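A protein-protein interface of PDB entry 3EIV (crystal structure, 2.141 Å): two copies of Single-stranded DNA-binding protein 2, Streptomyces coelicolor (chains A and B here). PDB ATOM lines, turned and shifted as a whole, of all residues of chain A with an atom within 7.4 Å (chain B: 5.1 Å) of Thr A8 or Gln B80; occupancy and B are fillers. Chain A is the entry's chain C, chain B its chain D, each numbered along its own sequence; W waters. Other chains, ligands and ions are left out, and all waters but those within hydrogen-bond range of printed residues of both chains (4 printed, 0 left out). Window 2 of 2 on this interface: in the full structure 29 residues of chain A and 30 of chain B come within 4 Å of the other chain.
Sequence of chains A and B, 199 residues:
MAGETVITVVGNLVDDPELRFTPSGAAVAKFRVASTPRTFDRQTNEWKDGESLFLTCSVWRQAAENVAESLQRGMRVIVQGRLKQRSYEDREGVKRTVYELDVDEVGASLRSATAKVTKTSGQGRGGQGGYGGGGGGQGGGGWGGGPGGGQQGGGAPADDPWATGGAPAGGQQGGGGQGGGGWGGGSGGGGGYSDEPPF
Of the 15 printed residues of chain A, 5 touch a printed residue of chain B. Along chain A the printed residues that touch a printed residue of chain B span positions 8 to 111. Of the 14 printed residues of chain B, 5 touch a printed residue of chain A.
Water W1 bridges O of Thr B8 (2.6 Å) and NE2 of Gln A80 (3.1 Å). Water W3 bridges the backbone carbonyl oxygen of Thr A8 (2.7 Å) and the side-chain amide nitrogen of Gln B80 (3.0 Å). Water W4 lies within hydrogen-bond range of OE1 of Gln B80 (2.8 Å) and O of Thr A8 (3.5 Å). Water W2 lies within hydrogen-bond range of OE1 of Gln A80 (3.1 Å) and O of Thr B8 (3.4 Å).
Thr B8 touches its own counterpart, Thr A8. Thr A8 touches Gln B80, and with the chains exchanged Gln A80 touches Thr B8. Ile A78 touches its own counterpart, Ile B78. Gln A80 touches Ile B78, but with the chains exchanged Ile A78 does not touch Gln B80 (4.04 Å). 9 positions are printed for both chains.
Thr A8 touches just these residues of chain B: Thr B8 (2.6 Å) and Gln B80 (3.6 Å). Printed residues of chain A within 4 Å of Gln B80: Thr A8 (3.6 Å). Of the printed residues of chain B, Val A10 touches Glu B105 (3.6 Å). Printed residues of chain B within 4 Å of Ile A78: Ile B78 (3.6 Å). Ile A7 touches none of the printed residues of chain B. The nearest printed residue of chain B that does not touch Thr A8 is Ile B78 (5.2 Å).
The backbone carbonyl oxygen of Val A10 sits at hydrogen-bond distance from the side-chain hydroxyl of Ser A35 (3.0 Å). O of Gln B80 sits at hydrogen-bond distance from N of Asp B104, at 2.8 Å. The backbone NH (N) of Gln B80 is in hydrogen-bond range of the backbone carbonyl oxygen (O) of Glu B105 (2.9 Å). The side-chain carboxylate of Asp B104 is in salt-bridge range of the guanidinium group of Arg B82, 2.6 Å away.
Among the printed residues, merely in contact across the chains: Ile A78 with Ile B78 (3.6 Å), Val A10 with Glu B105 (3.6 Å), Thr A8 with Gln B80 (3.6 Å), Gln A80 with Thr B8 (3.7 Å) and Gln A80 with Ile B78 (3.9 Å).
The guanidinium group (NH2) of Arg A111 is in salt-bridge range of the side-chain carboxylate (OE2) of Glu B105, at 3.0 Å. The side-chain hydroxyl of Thr A8 is in hydrogen-bond range of the side-chain hydroxyl of Thr B8 (2.6 Å). O of Asp B104 lies within hydrogen-bond range of NH2 of Arg A111, at 2.7 Å.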
ATOM      1  N   THR A   5      24.395  10.614  12.194  1.00  0.00           N
ATOM      2  CA  THR A   5      25.362  10.183  11.196  1.00  0.00           C
ATOM      3  C   THR A   5      24.654   9.967   9.860  1.00  0.00           C
ATOM      4  O   THR A   5      23.972   8.962   9.656  1.00  0.00           O
ATOM      5  CB  THR A   5      26.122   8.911  11.635  1.00  0.00           C
ATOM      6  OG1 THR A   5      26.722   9.136  12.916  1.00  0.00           O
ATOM      7  CG2 THR A   5      27.226   8.550  10.609  1.00  0.00           C
ATOM      8  N   VAL A   6      24.800  10.938   8.968  1.00  0.00           N
ATOM      9  CA  VAL A   6      24.140  10.896   7.670  1.00  0.00           C
ATOM     10  C   VAL A   6      25.071  10.296   6.627  1.00  0.00           C
ATOM     11  O   VAL A   6      26.223  10.698   6.505  1.00  0.00           O
ATOM     12  CB  VAL A   6      23.708  12.304   7.216  1.00  0.00           C
ATOM     13  CG1 VAL A   6      23.032  12.247   5.847  1.00  0.00           C
ATOM     14  CG2 VAL A   6      22.774  12.949   8.266  1.00  0.00           C
ATOM     15  N   ILE A   7      24.572   9.323   5.879  1.00  0.00           N
ATOM     16  CA  ILE A   7      25.383   8.679   4.857  1.00  0.00           C
ATOM     17  C   ILE A   7      24.619   8.491   3.557  1.00  0.00           C
ATOM     18  O   ILE A   7      23.388   8.472   3.537  1.00  0.00           O
ATOM     19  CB  ILE A   7      25.937   7.305   5.325  1.00  0.00           C
ATOM     20  CG1 ILE A   7      24.821   6.267   5.415  1.00  0.00           C
ATOM     21  CG2 ILE A   7      26.670   7.434   6.657  1.00  0.00           C
ATOM     22  CD1 ILE A   7      25.352   4.823   5.537  1.00  0.00           C
ATOM     23  N   THR A   8      25.372   8.356   2.471  1.00  0.00           N
ATOM     24  CA  THR A   8      24.803   8.074   1.168  1.00  0.00           C
ATOM     25  C   THR A   8      25.224   6.672   0.763  1.00  0.00           C
ATOM     26  O   THR A   8      26.405   6.327   0.833  1.00  0.00           O
ATOM     27  CB  THR A   8      25.294   9.083   0.114  1.00  0.00           C
ATOM     28  OG1 THR A   8      24.853  10.404   0.466  1.00  0.00           O
ATOM     29  CG2 THR A   8      24.753   8.719  -1.264  1.00  0.00           C
ATOM     30  N   VAL A   9      24.254   5.850   0.381  1.00  0.00           N
ATOM     31  CA  VAL A   9      24.546   4.502  -0.096  1.00  0.00           C
ATOM     32  C   VAL A   9      23.928   4.281  -1.484  1.00  0.00           C
ATOM     33  O   VAL A   9      22.819   4.748  -1.775  1.00  0.00           O
ATOM     34  CB  VAL A   9      24.028   3.399   0.882  1.00  0.00           C
ATOM     35  CG1 VAL A   9      24.472   2.009   0.414  1.00  0.00           C
ATOM     36  CG2 VAL A   9      24.532   3.653   2.282  1.00  0.00           C
ATOM     37  N   VAL A  10      24.652   3.553  -2.325  1.00  0.00           N
ATOM     38  CA  VAL A  10      24.225   3.268  -3.687  1.00  0.00           C
ATOM     39  C   VAL A  10      24.294   1.765  -3.928  1.00  0.00           C
ATOM     40  O   VAL A  10      25.321   1.139  -3.692  1.00  0.00           O
ATOM     41  CB  VAL A  10      25.168   3.960  -4.699  1.00  0.00           C
ATOM     42  CG1 VAL A  10      24.834   3.549  -6.121  1.00  0.00           C
ATOM     43  CG2 VAL A  10      25.112   5.468  -4.547  1.00  0.00           C
ATOM     44  N   SER A  35      25.298  -2.903  -1.714  1.00  0.00           N
ATOM     45  CA  SER A  35      26.257  -2.019  -2.360  1.00  0.00           C
ATOM     46  C   SER A  35      27.558  -2.779  -2.547  1.00  0.00           C
ATOM     47  O   SER A  35      28.169  -3.214  -1.566  1.00  0.00           O
ATOM     48  CB  SER A  35      26.481  -0.768  -1.495  1.00  0.00           C
ATOM     49  OG  SER A  35      27.552   0.027  -1.983  1.00  0.00           O
ATOM     50  N   LEU A  53      28.129  -4.626   0.737  1.00  0.00           N
ATOM     51  CA  LEU A  53      27.623  -4.018   1.954  1.00  0.00           C
ATOM     52  C   LEU A  53      26.096  -4.086   1.903  1.00  0.00           C
ATOM     53  O   LEU A  53      25.493  -3.599   0.951  1.00  0.00           O
ATOM     54  CB  LEU A  53      28.090  -2.565   2.013  1.00  0.00           C
ATOM     55  CG  LEU A  53      27.596  -1.662   3.147  1.00  0.00           C
ATOM     56  CD1 LEU A  53      27.994  -2.225   4.504  1.00  0.00           C
ATOM     57  CD2 LEU A  53      28.152  -0.255   2.971  1.00  0.00           C
ATOM     58  N   LEU A  55      22.469  -3.079   3.766  1.00  0.00           N
ATOM     59  CA  LEU A  55      21.793  -2.221   4.745  1.00  0.00           C
ATOM     60  C   LEU A  55      20.282  -2.292   4.583  1.00  0.00           C
ATOM     61  O   LEU A  55      19.749  -2.175   3.473  1.00  0.00           O
ATOM     62  CB  LEU A  55      22.250  -0.766   4.602  1.00  0.00           C
ATOM     63  CG  LEU A  55      23.255  -0.157   5.587  1.00  0.00           C
ATOM     64  CD1 LEU A  55      24.048  -1.211   6.355  1.00  0.00           C
ATOM     65  CD2 LEU A  55      24.189   0.808   4.861  1.00  0.00           C
ATOM     66  N   ILE A  78      19.971   5.219  -5.173  1.00  0.00           N
ATOM     67  CA  ILE A  78      20.839   6.025  -4.334  1.00  0.00           C
ATOM     68  C   ILE A  78      20.005   6.584  -3.172  1.00  0.00           C
ATOM     69  O   ILE A  78      18.962   7.211  -3.381  1.00  0.00           O
ATOM     70  CB  ILE A  78      21.507   7.165  -5.138  1.00  0.00           C
ATOM     71  CG1 ILE A  78      22.242   8.137  -4.208  1.00  0.00           C
ATOM     72  CG2 ILE A  78      20.478   7.904  -5.995  1.00  0.00           C
ATOM     73  CD1 ILE A  78      23.198   9.078  -4.956  1.00  0.00           C
ATOM     74  N   VAL A  79      20.459   6.322  -1.951  1.00  0.00           N
ATOM     75  CA  VAL A  79      19.738   6.728  -0.756  1.00  0.00           C
ATOM     76  C   VAL A  79      20.636   7.533   0.170  1.00  0.00           C
ATOM     77  O   VAL A  79      21.800   7.182   0.391  1.00  0.00           O
ATOM     78  CB  VAL A  79      19.186   5.505   0.011  1.00  0.00           C
ATOM     79  CG1 VAL A  79      18.272   4.692  -0.894  1.00  0.00           C
ATOM     80  CG2 VAL A  79      20.324   4.625   0.470  1.00  0.00           C
ATOM     81  N   GLN A  80      20.098   8.634   0.688  1.00  0.00           N
ATOM     82  CA  GLN A  80      20.756   9.372   1.749  1.00  0.00           C
ATOM     83  C   GLN A  80      19.889   9.265   3.000  1.00  0.00           C
ATOM     84  O   GLN A  80      18.660   9.329   2.921  1.00  0.00           O
ATOM     85  CB  GLN A  80      20.949  10.837   1.368  1.00  0.00           C
ATOM     86  CG  GLN A  80      21.597  11.669   2.467  1.00  0.00           C
ATOM     87  CD  GLN A  80      21.879  13.096   2.027  1.00  0.00           C
ATOM     88  OE1 GLN A  80      20.985  13.797   1.574  1.00  0.00           O
ATOM     89  NE2 GLN A  80      23.124  13.531   2.169  1.00  0.00           N
ATOM     90  N   GLY A  81      20.518   9.083   4.154  1.00  0.00           N
ATOM     91  CA  GLY A  81      19.752   8.961   5.381  1.00  0.00           C
ATOM     92  C   GLY A  81      20.612   8.797   6.613  1.00  0.00           C
ATOM     93  O   GLY A  81      21.839   8.888   6.549  1.00  0.00           O
ATOM     94  N   LEU A 101      19.188   2.015   7.982  1.00  0.00           N
ATOM     95  CA  LEU A 101      19.257   3.361   7.432  1.00  0.00           C
ATOM     96  C   LEU A 101      17.869   3.988   7.467  1.00  0.00           C
ATOM     97  O   LEU A 101      16.952   3.513   6.801  1.00  0.00           O
ATOM     98  CB  LEU A 101      19.777   3.345   5.987  1.00  0.00           C
ATOM     99  CG  LEU A 101      20.928   4.275   5.561  1.00  0.00           C
ATOM    100  CD1 LEU A 101      20.975   4.438   4.027  1.00  0.00           C
ATOM    101  CD2 LEU A 101      20.870   5.628   6.219  1.00  0.00           C
ATOM    102  N   ARG A 111      22.107   5.534 -13.733  1.00  0.00           N
ATOM    103  CA  ARG A 111      23.379   5.027 -14.233  1.00  0.00           C
ATOM    104  C   ARG A 111      23.190   4.119 -15.452  1.00  0.00           C
ATOM    105  O   ARG A 111      23.924   4.220 -16.442  1.00  0.00           O
ATOM    106  CB  ARG A 111      24.162   4.265 -13.156  1.00  0.00           C
ATOM    107  CG  ARG A 111      25.400   3.549 -13.747  1.00  0.00           C
ATOM    108  CD  ARG A 111      26.285   2.910 -12.681  1.00  0.00           C
ATOM    109  NE  ARG A 111      26.849   3.916 -11.784  1.00  0.00           N
ATOM    110  CZ  ARG A 111      28.081   4.404 -11.886  1.00  0.00           C
ATOM    111  NH1 ARG A 111      28.890   3.970 -12.846  1.00  0.00           N
ATOM    112  NH2 ARG A 111      28.505   5.322 -11.027  1.00  0.00           N
ATOM    113  N   VAL B   6      34.199  14.330  -1.859  1.00  0.00           N
ATOM    114  CA  VAL B   6      32.940  13.694  -2.235  1.00  0.00           C
ATOM    115  C   VAL B   6      31.786  14.297  -1.443  1.00  0.00           C
ATOM    116  O   VAL B   6      31.868  14.421  -0.231  1.00  0.00           O
ATOM    117  CB  VAL B   6      32.987  12.170  -1.984  1.00  0.00           C
ATOM    118  CG1 VAL B   6      31.627  11.530  -2.247  1.00  0.00           C
ATOM    119  CG2 VAL B   6      34.084  11.518  -2.838  1.00  0.00           C
ATOM    120  N   ILE B   7      30.713  14.668  -2.135  1.00  0.00           N
ATOM    121  CA  ILE B   7      29.534  15.202  -1.477  1.00  0.00           C
ATOM    122  C   ILE B   7      28.235  14.711  -2.104  1.00  0.00           C
ATOM    123  O   ILE B   7      28.208  14.231  -3.250  1.00  0.00           O
ATOM    124  CB  ILE B   7      29.533  16.753  -1.472  1.00  0.00           C
ATOM    125  CG1 ILE B   7      29.314  17.316  -2.883  1.00  0.00           C
ATOM    126  CG2 ILE B   7      30.847  17.296  -0.905  1.00  0.00           C
ATOM    127  CD1 ILE B   7      28.949  18.818  -2.858  1.00  0.00           C
ATOM    128  N   THR B   8      27.153  14.849  -1.347  1.00  0.00           N
ATOM    129  CA  THR B   8      25.829  14.515  -1.844  1.00  0.00           C
ATOM    130  C   THR B   8      24.995  15.803  -1.843  1.00  0.00           C
ATOM    131  O   THR B   8      25.066  16.579  -0.905  1.00  0.00           O
ATOM    132  CB  THR B   8      25.166  13.440  -0.966  1.00  0.00           C
ATOM    133  OG1 THR B   8      25.941  12.238  -1.023  1.00  0.00           O
ATOM    134  CG2 THR B   8      23.749  13.138  -1.439  1.00  0.00           C
ATOM    135  N   VAL B   9      24.254  16.052  -2.919  1.00  0.00           N
ATOM    136  CA  VAL B   9      23.362  17.203  -2.981  1.00  0.00           C
ATOM    137  C   VAL B   9      21.985  16.741  -3.430  1.00  0.00           C
ATOM    138  O   VAL B   9      21.854  15.842  -4.272  1.00  0.00           O
ATOM    139  CB  VAL B   9      23.864  18.294  -3.968  1.00  0.00           C
ATOM    140  CG1 VAL B   9      22.898  19.482  -3.987  1.00  0.00           C
ATOM    141  CG2 VAL B   9      25.266  18.756  -3.599  1.00  0.00           C
ATOM    142  N   ILE B  78      18.790  13.496  -6.675  1.00  0.00           N
ATOM    143  CA  ILE B  78      19.831  13.327  -5.681  1.00  0.00           C
ATOM    144  C   ILE B  78      21.120  12.942  -6.415  1.00  0.00           C
ATOM    145  O   ILE B  78      21.145  11.980  -7.193  1.00  0.00           O
ATOM    146  CB  ILE B  78      19.450  12.274  -4.602  1.00  0.00           C
ATOM    147  CG1 ILE B  78      20.678  11.866  -3.780  1.00  0.00           C
ATOM    148  CG2 ILE B  78      18.882  11.031  -5.249  1.00  0.00           C
ATOM    149  CD1 ILE B  78      20.319  11.211  -2.461  1.00  0.00           C
ATOM    150  N   VAL B  79      22.178  13.706  -6.195  1.00  0.00           N
ATOM    151  CA  VAL B  79      23.448  13.435  -6.865  1.00  0.00           C
ATOM    152  C   VAL B  79      24.605  13.300  -5.883  1.00  0.00           C
ATOM    153  O   VAL B  79      24.713  14.058  -4.903  1.00  0.00           O
ATOM    154  CB  VAL B  79      23.812  14.531  -7.879  1.00  0.00           C
ATOM    155  CG1 VAL B  79      22.925  14.441  -9.109  1.00  0.00           C
ATOM    156  CG2 VAL B  79      23.688  15.898  -7.242  1.00  0.00           C
ATOM    157  N   GLN B  80      25.475  12.329  -6.148  1.00  0.00           N
ATOM    158  CA  GLN B  80      26.710  12.213  -5.389  1.00  0.00           C
ATOM    159  C   GLN B  80      27.868  12.336  -6.360  1.00  0.00           C
ATOM    160  O   GLN B  80      27.872  11.708  -7.427  1.00  0.00           O
ATOM    161  CB  GLN B  80      26.778  10.906  -4.600  1.00  0.00           C
ATOM    162  CG  GLN B  80      28.108  10.714  -3.822  1.00  0.00           C
ATOM    163  CD  GLN B  80      28.105   9.467  -2.929  1.00  0.00           C
ATOM    164  OE1 GLN B  80      27.799   8.369  -3.386  1.00  0.00           O
ATOM    165  NE2 GLN B  80      28.442   9.645  -1.645  1.00  0.00           N
ATOM    166  N   GLY B  81      28.857  13.139  -5.998  1.00  0.00           N
ATOM    167  CA  GLY B  81      30.006  13.313  -6.864  1.00  0.00           C
ATOM    168  C   GLY B  81      31.148  14.022  -6.182  1.00  0.00           C
ATOM    169  O   GLY B  81      31.220  14.066  -4.958  1.00  0.00           O
ATOM    170  N   ARG B  82      32.043  14.580  -6.988  1.00  0.00           N
ATOM    171  CA  ARG B  82      33.241  15.222  -6.474  1.00  0.00           C
ATOM    172  C   ARG B  82      33.222  16.722  -6.731  1.00  0.00           C
ATOM    173  O   ARG B  82      33.110  17.173  -7.875  1.00  0.00           O
ATOM    174  CB  ARG B  82      34.496  14.560  -7.056  1.00  0.00           C
ATOM    175  CG  ARG B  82      34.805  13.231  -6.384  1.00  0.00           C
ATOM    176  CD  ARG B  82      35.473  12.227  -7.315  1.00  0.00           C
ATOM    177  NE  ARG B  82      34.592  11.872  -8.421  1.00  0.00           N
ATOM    178  CZ  ARG B  82      34.868  12.111  -9.696  1.00  0.00           C
ATOM    179  NH1 ARG B  82      34.002  11.757 -10.637  1.00  0.00           N
ATOM    180  NH2 ARG B  82      36.021  12.688 -10.032  1.00  0.00           N
ATOM    181  N   LEU B 101      30.280  20.153  -9.670  1.00  0.00           N
ATOM    182  CA  LEU B 101      30.112  18.807  -9.172  1.00  0.00           C
ATOM    183  C   LEU B 101      30.345  17.818 -10.326  1.00  0.00           C
ATOM    184  O   LEU B 101      29.605  17.801 -11.303  1.00  0.00           O
ATOM    185  CB  LEU B 101      28.718  18.648  -8.547  1.00  0.00           C
ATOM    186  CG  LEU B 101      28.383  17.395  -7.726  1.00  0.00           C
ATOM    187  CD1 LEU B 101      29.403  17.144  -6.616  1.00  0.00           C
ATOM    188  CD2 LEU B 101      26.962  17.491  -7.136  1.00  0.00           C
ATOM    189  N   ASP B 102      31.404  17.028 -10.222  1.00  0.00           N
ATOM    190  CA  ASP B 102      31.613  15.910 -11.134  1.00  0.00           C
ATOM    191  C   ASP B 102      30.843  14.726 -10.586  1.00  0.00           C
ATOM    192  O   ASP B 102      31.276  14.097  -9.627  1.00  0.00           O
ATOM    193  CB  ASP B 102      33.099  15.544 -11.222  1.00  0.00           C
ATOM    194  CG  ASP B 102      33.857  16.388 -12.232  1.00  0.00           C
ATOM    195  OD1 ASP B 102      33.242  17.259 -12.881  1.00  0.00           O
ATOM    196  OD2 ASP B 102      35.079  16.176 -12.380  1.00  0.00           O
ATOM    197  N   VAL B 103      29.711  14.425 -11.203  1.00  0.00           N
ATOM    198  CA  VAL B 103      28.753  13.465 -10.658  1.00  0.00           C
ATOM    199  C   VAL B 103      29.168  12.014 -10.902  1.00  0.00           C
ATOM    200  O   VAL B 103      29.523  11.640 -12.020  1.00  0.00           O
ATOM    201  CB  VAL B 103      27.353  13.713 -11.256  1.00  0.00           C
ATOM    202  CG1 VAL B 103      26.353  12.671 -10.774  1.00  0.00           C
ATOM    203  CG2 VAL B 103      26.880  15.130 -10.934  1.00  0.00           C
ATOM    204  N   ASP B 104      29.139  11.205  -9.843  1.00  0.00           N
ATOM    205  CA  ASP B 104      29.386   9.765  -9.957  1.00  0.00           C
ATOM    206  C   ASP B 104      28.071   8.984  -9.988  1.00  0.00           C
ATOM    207  O   ASP B 104      27.982   7.905 -10.582  1.00  0.00           O
ATOM    208  CB  ASP B 104      30.239   9.267  -8.786  1.00  0.00           C
ATOM    209  CG  ASP B 104      31.629   9.871  -8.777  1.00  0.00           C
ATOM    210  OD1 ASP B 104      32.098  10.263  -7.690  1.00  0.00           O
ATOM    211  OD2 ASP B 104      32.252   9.967  -9.854  1.00  0.00           O
ATOM    212  N   GLU B 105      27.053   9.526  -9.329  1.00  0.00           N
ATOM    213  CA  GLU B 105      25.761   8.858  -9.283  1.00  0.00           C
ATOM    214  C   GLU B 105      24.626   9.873  -9.296  1.00  0.00           C
ATOM    215  O   GLU B 105      24.662  10.866  -8.561  1.00  0.00           O
ATOM    216  CB  GLU B 105      25.678   7.967  -8.037  1.00  0.00           C
ATOM    217  CG  GLU B 105      24.589   6.909  -8.111  1.00  0.00           C
ATOM    218  CD  GLU B 105      25.005   5.732  -8.997  1.00  0.00           C
ATOM    219  OE1 GLU B 105      24.122   5.089  -9.604  1.00  0.00           O
ATOM    220  OE2 GLU B 105      26.219   5.454  -9.075  1.00  0.00           O
HETATM  221  O   HOH W   1      24.822  16.091   1.650  1.00  0.00           O
HETATM  222  O   HOH W   2      22.323  16.581   1.069  1.00  0.00           O
HETATM  223  O   HOH W   3      28.894   7.145   0.026  1.00  0.00           O
HETATM  224  O   HOH W   4      28.282   5.914  -2.052  1.00  0.00           O
